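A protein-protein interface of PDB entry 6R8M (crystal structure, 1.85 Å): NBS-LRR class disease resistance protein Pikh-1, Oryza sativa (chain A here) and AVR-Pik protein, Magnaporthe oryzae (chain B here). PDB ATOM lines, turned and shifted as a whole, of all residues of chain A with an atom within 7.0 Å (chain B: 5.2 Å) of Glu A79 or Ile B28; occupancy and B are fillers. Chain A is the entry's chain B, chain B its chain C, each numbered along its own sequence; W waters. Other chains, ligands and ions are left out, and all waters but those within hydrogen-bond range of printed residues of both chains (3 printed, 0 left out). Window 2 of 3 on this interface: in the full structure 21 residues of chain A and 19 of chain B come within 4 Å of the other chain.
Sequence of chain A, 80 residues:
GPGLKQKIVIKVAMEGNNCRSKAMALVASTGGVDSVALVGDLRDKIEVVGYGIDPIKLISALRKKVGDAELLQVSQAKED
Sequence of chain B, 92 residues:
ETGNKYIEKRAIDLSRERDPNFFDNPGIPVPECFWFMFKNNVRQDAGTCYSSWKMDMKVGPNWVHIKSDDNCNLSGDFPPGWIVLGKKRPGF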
ATOM      1  N   PRO A   2     -16.434  13.912  23.781  1.00  0.00           N
ATOM      2  CA  PRO A   2     -15.263  13.644  24.620  1.00  0.00           C
ATOM      3  C   PRO A   2     -15.119  12.182  25.090  1.00  0.00           C
ATOM      4  O   PRO A   2     -14.195  11.933  25.849  1.00  0.00           O
ATOM      5  CB  PRO A   2     -15.566  14.571  25.811  1.00  0.00           C
ATOM      6  CG  PRO A   2     -17.082  14.455  25.993  1.00  0.00           C
ATOM      7  CD  PRO A   2     -17.635  14.157  24.605  1.00  0.00           C
ATOM      8  N   GLY A   3     -16.011  11.283  24.636  1.00  0.00           N
ATOM      9  CA  GLY A   3     -16.116   9.860  25.039  1.00  0.00           C
ATOM     10  C   GLY A   3     -14.816   9.092  24.851  1.00  0.00           C
ATOM     11  O   GLY A   3     -14.171   9.222  23.779  1.00  0.00           O
ATOM     12  N   LEU A   4     -14.412   8.328  25.870  1.00  0.00           N
ATOM     13  CA  LEU A   4     -13.086   7.669  25.900  1.00  0.00           C
ATOM     14  C   LEU A   4     -13.209   6.366  25.098  1.00  0.00           C
ATOM     15  O   LEU A   4     -14.325   5.811  24.979  1.00  0.00           O
ATOM     16  CB  LEU A   4     -12.620   7.416  27.349  1.00  0.00           C
ATOM     17  CG  LEU A   4     -12.279   8.631  28.229  1.00  0.00           C
ATOM     18  CD1 LEU A   4     -11.900   8.199  29.647  1.00  0.00           C
ATOM     19  CD2 LEU A   4     -11.159   9.468  27.636  1.00  0.00           C
ATOM     20  N   LYS A   5     -12.094   5.886  24.564  1.00  0.00           N
ATOM     21  CA  LYS A   5     -12.073   4.581  23.892  1.00  0.00           C
ATOM     22  C   LYS A   5     -12.121   3.519  24.989  1.00  0.00           C
ATOM     23  O   LYS A   5     -11.589   3.735  26.097  1.00  0.00           O
ATOM     24  CB  LYS A   5     -10.850   4.459  22.977  1.00  0.00           C
ATOM     25  CG  LYS A   5     -10.865   5.378  21.746  1.00  0.00           C
ATOM     26  CD  LYS A   5     -12.165   5.383  20.957  1.00  0.00           C
ATOM     27  CE  LYS A   5     -12.214   6.378  19.807  1.00  0.00           C
ATOM     28  NZ  LYS A   5     -11.320   5.978  18.697  1.00  0.00           N
ATOM     29  N   GLN A   6     -12.725   2.405  24.630  1.00  0.00           N
ATOM     30  CA  GLN A   6     -12.742   1.142  25.372  1.00  0.00           C
ATOM     31  C   GLN A   6     -11.535   0.262  25.041  1.00  0.00           C
ATOM     32  O   GLN A   6     -11.105   0.205  23.857  1.00  0.00           O
ATOM     33  CB  GLN A   6     -13.974   0.357  24.925  1.00  0.00           C
ATOM     34  CG  GLN A   6     -15.307   1.032  25.227  1.00  0.00           C
ATOM     35  CD  GLN A   6     -16.399   0.238  24.539  1.00  0.00           C
ATOM     36  OE1 GLN A   6     -16.524   0.235  23.310  1.00  0.00           O
ATOM     37  NE2 GLN A   6     -17.094  -0.572  25.318  1.00  0.00           N
ATOM     38  N   LYS A   7     -11.092  -0.484  26.041  1.00  0.00           N
ATOM     39  CA  LYS A   7     -10.157  -1.591  25.871  1.00  0.00           C
ATOM     40  C   LYS A   7     -10.846  -2.815  26.475  1.00  0.00           C
ATOM     41  O   LYS A   7     -11.301  -2.763  27.665  1.00  0.00           O
ATOM     42  CB  LYS A   7      -8.826  -1.338  26.554  1.00  0.00           C
ATOM     43  CG  LYS A   7      -7.851  -2.498  26.379  1.00  0.00           C
ATOM     44  CD  LYS A   7      -6.556  -2.299  27.088  1.00  0.00           C
ATOM     45  CE  LYS A   7      -5.812  -1.053  26.660  1.00  0.00           C
ATOM     46  NZ  LYS A   7      -4.543  -0.935  27.415  1.00  0.00           N
ATOM     47  N   ASP A  34     -11.638  -0.405  16.557  1.00  0.00           N
ATOM     48  CA  ASP A  34     -10.455   0.283  15.970  1.00  0.00           C
ATOM     49  C   ASP A  34      -9.318  -0.717  15.732  1.00  0.00           C
ATOM     50  O   ASP A  34      -8.559  -0.551  14.747  1.00  0.00           O
ATOM     51  CB  ASP A  34      -9.884   1.378  16.877  1.00  0.00           C
ATOM     52  CG  ASP A  34     -10.780   2.596  17.060  1.00  0.00           C
ATOM     53  OD1 ASP A  34     -11.755   2.740  16.284  1.00  0.00           O
ATOM     54  OD2 ASP A  34     -10.497   3.395  18.010  1.00  0.00           O
ATOM     55  N   SER A  35      -9.112  -1.655  16.643  1.00  0.00           N
ATOM     56  CA  SER A  35      -7.996  -2.614  16.532  1.00  0.00           C
ATOM     57  C   SER A  35      -8.296  -3.914  17.267  1.00  0.00           C
ATOM     58  O   SER A  35      -9.069  -3.919  18.217  1.00  0.00           O
ATOM     59  CB  SER A  35      -6.709  -2.011  16.982  1.00  0.00           C
ATOM     60  OG  SER A  35      -6.702  -1.765  18.372  1.00  0.00           O
ATOM     61  N   GLU A  47      -6.837  -8.425  22.441  1.00  0.00           N
ATOM     62  CA  GLU A  47      -7.051  -7.050  22.966  1.00  0.00           C
ATOM     63  C   GLU A  47      -7.757  -6.266  21.874  1.00  0.00           C
ATOM     64  O   GLU A  47      -7.263  -6.203  20.743  1.00  0.00           O
ATOM     65  CB  GLU A  47      -5.736  -6.412  23.440  1.00  0.00           C
ATOM     66  CG  GLU A  47      -5.934  -5.015  23.945  1.00  0.00           C
ATOM     67  CD  GLU A  47      -4.694  -4.317  24.501  1.00  0.00           C
ATOM     68  OE1 GLU A  47      -4.554  -3.108  24.232  1.00  0.00           O
ATOM     69  OE2 GLU A  47      -3.905  -4.957  25.206  1.00  0.00           O
ATOM     70  N   VAL A  49      -9.608  -2.560  20.907  1.00  0.00           N
ATOM     71  CA  VAL A  49      -9.800  -1.126  21.222  1.00  0.00           C
ATOM     72  C   VAL A  49     -10.880  -0.591  20.296  1.00  0.00           C
ATOM     73  O   VAL A  49     -10.835  -0.876  19.085  1.00  0.00           O
ATOM     74  CB  VAL A  49      -8.469  -0.356  21.131  1.00  0.00           C
ATOM     75  CG1 VAL A  49      -8.688   1.132  21.339  1.00  0.00           C
ATOM     76  CG2 VAL A  49      -7.459  -0.904  22.123  1.00  0.00           C
ATOM     77  N   GLN A  76     -10.774   1.753  30.109  1.00  0.00           N
ATOM     78  CA  GLN A  76     -10.879   2.925  29.218  1.00  0.00           C
ATOM     79  C   GLN A  76      -9.468   3.382  28.904  1.00  0.00           C
ATOM     80  O   GLN A  76      -8.539   3.183  29.727  1.00  0.00           O
ATOM     81  CB  GLN A  76     -11.673   4.049  29.874  1.00  0.00           C
ATOM     82  CG  GLN A  76     -13.055   3.673  30.334  1.00  0.00           C
ATOM     83  CD  GLN A  76     -13.686   4.940  30.846  1.00  0.00           C
ATOM     84  OE1 GLN A  76     -13.310   5.444  31.909  1.00  0.00           O
ATOM     85  NE2 GLN A  76     -14.608   5.480  30.062  1.00  0.00           N
ATOM     86  N   ALA A  77      -9.296   3.981  27.744  1.00  0.00           N
ATOM     87  CA  ALA A  77      -8.013   4.587  27.357  1.00  0.00           C
ATOM     88  C   ALA A  77      -7.887   5.919  28.116  1.00  0.00           C
ATOM     89  O   ALA A  77      -8.863   6.687  28.134  1.00  0.00           O
ATOM     90  CB  ALA A  77      -7.951   4.788  25.871  1.00  0.00           C
ATOM     91  N   LYS A  78      -6.740   6.145  28.748  1.00  0.00           N
ATOM     92  CA  LYS A  78      -6.430   7.417  29.459  1.00  0.00           C
ATOM     93  C   LYS A  78      -6.027   8.426  28.385  1.00  0.00           C
ATOM     94  O   LYS A  78      -4.869   8.356  27.937  1.00  0.00           O
ATOM     95  CB  LYS A  78      -5.330   7.208  30.506  1.00  0.00           C
ATOM     96  CG  LYS A  78      -5.002   8.448  31.346  1.00  0.00           C
ATOM     97  CD  LYS A  78      -3.841   8.276  32.334  1.00  0.00           C
ATOM     98  CE  LYS A  78      -2.512   8.103  31.632  1.00  0.00           C
ATOM     99  NZ  LYS A  78      -1.369   8.019  32.565  1.00  0.00           N
ATOM    100  N   GLU A  79      -6.958   9.279  27.958  1.00  0.00           N
ATOM    101  CA  GLU A  79      -6.730  10.274  26.865  1.00  0.00           C
ATOM    102  C   GLU A  79      -6.654  11.690  27.438  1.00  0.00           C
ATOM    103  O   GLU A  79      -7.093  12.640  26.758  1.00  0.00           O
ATOM    104  CB  GLU A  79      -7.840  10.157  25.823  1.00  0.00           C
ATOM    105  CG  GLU A  79      -7.886   8.785  25.181  1.00  0.00           C
ATOM    106  CD  GLU A  79      -8.788   8.719  23.963  1.00  0.00           C
ATOM    107  OE1 GLU A  79     -10.010   8.477  24.145  1.00  0.00           O
ATOM    108  OE2 GLU A  79      -8.266   8.941  22.839  1.00  0.00           O
ATOM    109  N   ASP A  80      -6.095  11.812  28.643  1.00  0.00           N
ATOM    110  CA  ASP A  80      -5.954  13.082  29.407  1.00  0.00           C
ATOM    111  C   ASP A  80      -4.483  13.181  29.837  1.00  0.00           C
ATOM    112  O   ASP A  80      -3.859  14.223  29.625  1.00  0.00           O
ATOM    113  CB  ASP A  80      -6.991  13.184  30.544  1.00  0.00           C
ATOM    114  CG  ASP A  80      -7.276  11.899  31.324  1.00  0.00           C
ATOM    115  OD1 ASP A  80      -6.575  11.660  32.330  1.00  0.00           O
ATOM    116  OD2 ASP A  80      -8.213  11.145  30.932  1.00  0.00           O
ATOM    117  OXT ASP A  80      -3.887  12.225  30.363  1.00  0.00           O
ATOM    118  N   ASN B  25      -2.127   0.244  20.576  1.00  0.00           N
ATOM    119  CA  ASN B  25      -3.025   0.842  19.567  1.00  0.00           C
ATOM    120  C   ASN B  25      -2.469   2.231  19.210  1.00  0.00           C
ATOM    121  O   ASN B  25      -2.172   3.026  20.097  1.00  0.00           O
ATOM    122  CB  ASN B  25      -4.460   0.906  20.054  1.00  0.00           C
ATOM    123  CG  ASN B  25      -5.377   1.619  19.081  1.00  0.00           C
ATOM    124  OD1 ASN B  25      -5.478   2.862  19.099  1.00  0.00           O
ATOM    125  ND2 ASN B  25      -6.116   0.847  18.305  1.00  0.00           N
ATOM    126  N   PRO B  26      -2.226   2.540  17.916  1.00  0.00           N
ATOM    127  CA  PRO B  26      -1.630   3.830  17.529  1.00  0.00           C
ATOM    128  C   PRO B  26      -2.531   5.071  17.680  1.00  0.00           C
ATOM    129  O   PRO B  26      -2.000   6.142  17.706  1.00  0.00           O
ATOM    130  CB  PRO B  26      -1.233   3.622  16.057  1.00  0.00           C
ATOM    131  CG  PRO B  26      -2.182   2.562  15.580  1.00  0.00           C
ATOM    132  CD  PRO B  26      -2.409   1.638  16.773  1.00  0.00           C
ATOM    133  N   GLY B  27      -3.838   4.924  17.862  1.00  0.00           N
ATOM    134  CA  GLY B  27      -4.762   6.069  17.977  1.00  0.00           C
ATOM    135  C   GLY B  27      -5.000   6.472  19.422  1.00  0.00           C
ATOM    136  O   GLY B  27      -5.855   7.330  19.647  1.00  0.00           O
ATOM    137  N   ILE B  28      -4.363   5.809  20.397  1.00  0.00           N
ATOM    138  CA  ILE B  28      -4.543   6.165  21.831  1.00  0.00           C
ATOM    139  C   ILE B  28      -3.164   6.270  22.452  1.00  0.00           C
ATOM    140  O   ILE B  28      -2.179   5.720  21.965  1.00  0.00           O
ATOM    141  CB  ILE B  28      -5.477   5.186  22.582  1.00  0.00           C
ATOM    142  CG1 ILE B  28      -4.946   3.754  22.559  1.00  0.00           C
ATOM    143  CG2 ILE B  28      -6.903   5.276  22.050  1.00  0.00           C
ATOM    144  CD1 ILE B  28      -5.733   2.799  23.417  1.00  0.00           C
ATOM    145  N   PRO B  29      -3.026   7.018  23.553  1.00  0.00           N
ATOM    146  CA  PRO B  29      -1.726   7.160  24.186  1.00  0.00           C
ATOM    147  C   PRO B  29      -1.140   5.809  24.613  1.00  0.00           C
ATOM    148  O   PRO B  29      -1.904   4.914  24.999  1.00  0.00           O
ATOM    149  CB  PRO B  29      -2.033   8.065  25.397  1.00  0.00           C
ATOM    150  CG  PRO B  29      -3.264   8.833  24.990  1.00  0.00           C
ATOM    151  CD  PRO B  29      -4.079   7.814  24.215  1.00  0.00           C
ATOM    152  N   VAL B  30       0.184   5.707  24.566  1.00  0.00           N
ATOM    153  CA  VAL B  30       0.921   4.468  24.925  1.00  0.00           C
ATOM    154  C   VAL B  30       0.814   4.270  26.439  1.00  0.00           C
ATOM    155  O   VAL B  30       1.134   5.156  27.213  1.00  0.00           O
ATOM    156  CB  VAL B  30       2.375   4.527  24.438  1.00  0.00           C
ATOM    157  CG1 VAL B  30       3.137   3.260  24.806  1.00  0.00           C
ATOM    158  CG2 VAL B  30       2.441   4.799  22.937  1.00  0.00           C
ATOM    159  N   TYR B  50      -2.121   1.772  31.956  1.00  0.00           N
ATOM    160  CA  TYR B  50      -1.776   3.201  32.167  1.00  0.00           C
ATOM    161  C   TYR B  50      -1.365   3.396  33.629  1.00  0.00           C
ATOM    162  O   TYR B  50      -1.892   2.680  34.516  1.00  0.00           O
ATOM    163  CB  TYR B  50      -2.963   4.076  31.810  1.00  0.00           C
ATOM    164  CG  TYR B  50      -3.290   4.109  30.348  1.00  0.00           C
ATOM    165  CD1 TYR B  50      -2.517   4.866  29.476  1.00  0.00           C
ATOM    166  CD2 TYR B  50      -4.340   3.356  29.830  1.00  0.00           C
ATOM    167  CE1 TYR B  50      -2.803   4.913  28.132  1.00  0.00           C
ATOM    168  CE2 TYR B  50      -4.603   3.345  28.463  1.00  0.00           C
ATOM    169  CZ  TYR B  50      -3.833   4.130  27.621  1.00  0.00           C
ATOM    170  OH  TYR B  50      -4.074   4.157  26.288  1.00  0.00           O
HETATM  171  O   HOH W   1      -7.754   4.110  18.485  1.00  0.00           O
HETATM  172  O   HOH W   2      -3.800   1.262  26.042  1.00  0.00           O
HETATM  173  O   HOH W   3      -6.675   2.023  15.747  1.00  0.00           O
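Hydrophobic or aromatic side chains of chain A that line the printed part of chain B: Val A49 and Ala A77.
Of the 7 printed residues of chain B, 4 touch a printed residue of chain A.
Hydrophobic or aromatic side chains of chain B that line the printed part of chain A: Ile B28, Pro B29 and Tyr B50.
Among the printed residues, 9 pairs touch across the chains.
OG of Ser A35 is in hydrogen-bond range of ND2 of Asn B25, 2.7 Å away.
Printed residues of chain B within 4 Å of Val A49: Asn B25 and Ile B28.
Printed residues of chain B within 4 Å of Glu A79: Ile B28 (3.99 Å).
Of the printed residues of chain A, Asn B25 touches Ser A35 (2.7 Å) and Val A49 (3.9 Å).
No residue of chain A comes within 4 Å of Gly B27.
Of the printed residues of chain A, Ile B28 touches Lys A5 (3.97 Å), Val A49 (3.98 Å), Ala A77 (3.9 Å) and Glu A79 (3.99 Å).
Of the printed residues of chain A, Pro B29 touches Lys A78.
The nearest printed residue of chain A that does not touch Ile B28 is Lys A7 (5.0 Å).
Ile B28 touches Lys A5 (CG2 to CG, 3.97 Å).
CB of Val A49 touches ND2 of Asn B25, at 3.9 Å.
Ile B28 touches Val A49 (CD1 to CG1, 3.98 Å).
Ala A77 touches Ile B28 (CB to CD1, 3.9 Å).
Ala A77 touches Tyr B50.
CG of Pro B29 touches O of Lys A78, 3.4 Å away.
Tyr B50 touches Lys A78 (CE2 to N, 3.5 Å).
Ile B28 touches Glu A79.
Water W1 lies within hydrogen-bond range of OD1 of Asn B25 and OD2 of Asp A34.
Water W2 bridges the side-chain amino group of Lys A7 and the side-chain hydroxyl of Tyr B50.
Water W3 bridges the side-chain amide nitrogen (ND2) of Asn B25 (2.9 Å) and the backbone carbonyl oxygen (O) of Asp A34 (3.3 Å).
NZ of Lys A5 is in salt-bridge range of OD2 of Asp A34 (2.8 Å).
The backbone carbonyl oxygen of Lys A5 is in hydrogen-bond range of the backbone NH of Ala A77, 2.8 Å away.
N of Lys A5 lies within hydrogen-bond range of OE1 of Glu A79.
The backbone carbonyl oxygen of Ser A35 lies within hydrogen-bond range of the backbone NH of Val A49, at 3.1 Å.
OD1 of Asn B25 sits at hydrogen-bond distance from N of Ile B28 (3.4 Å).
The side-chain hydroxyl of Tyr B50 is in hydrogen-bond range of the backbone carbonyl oxygen of Pro B29 (2.6 Å).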
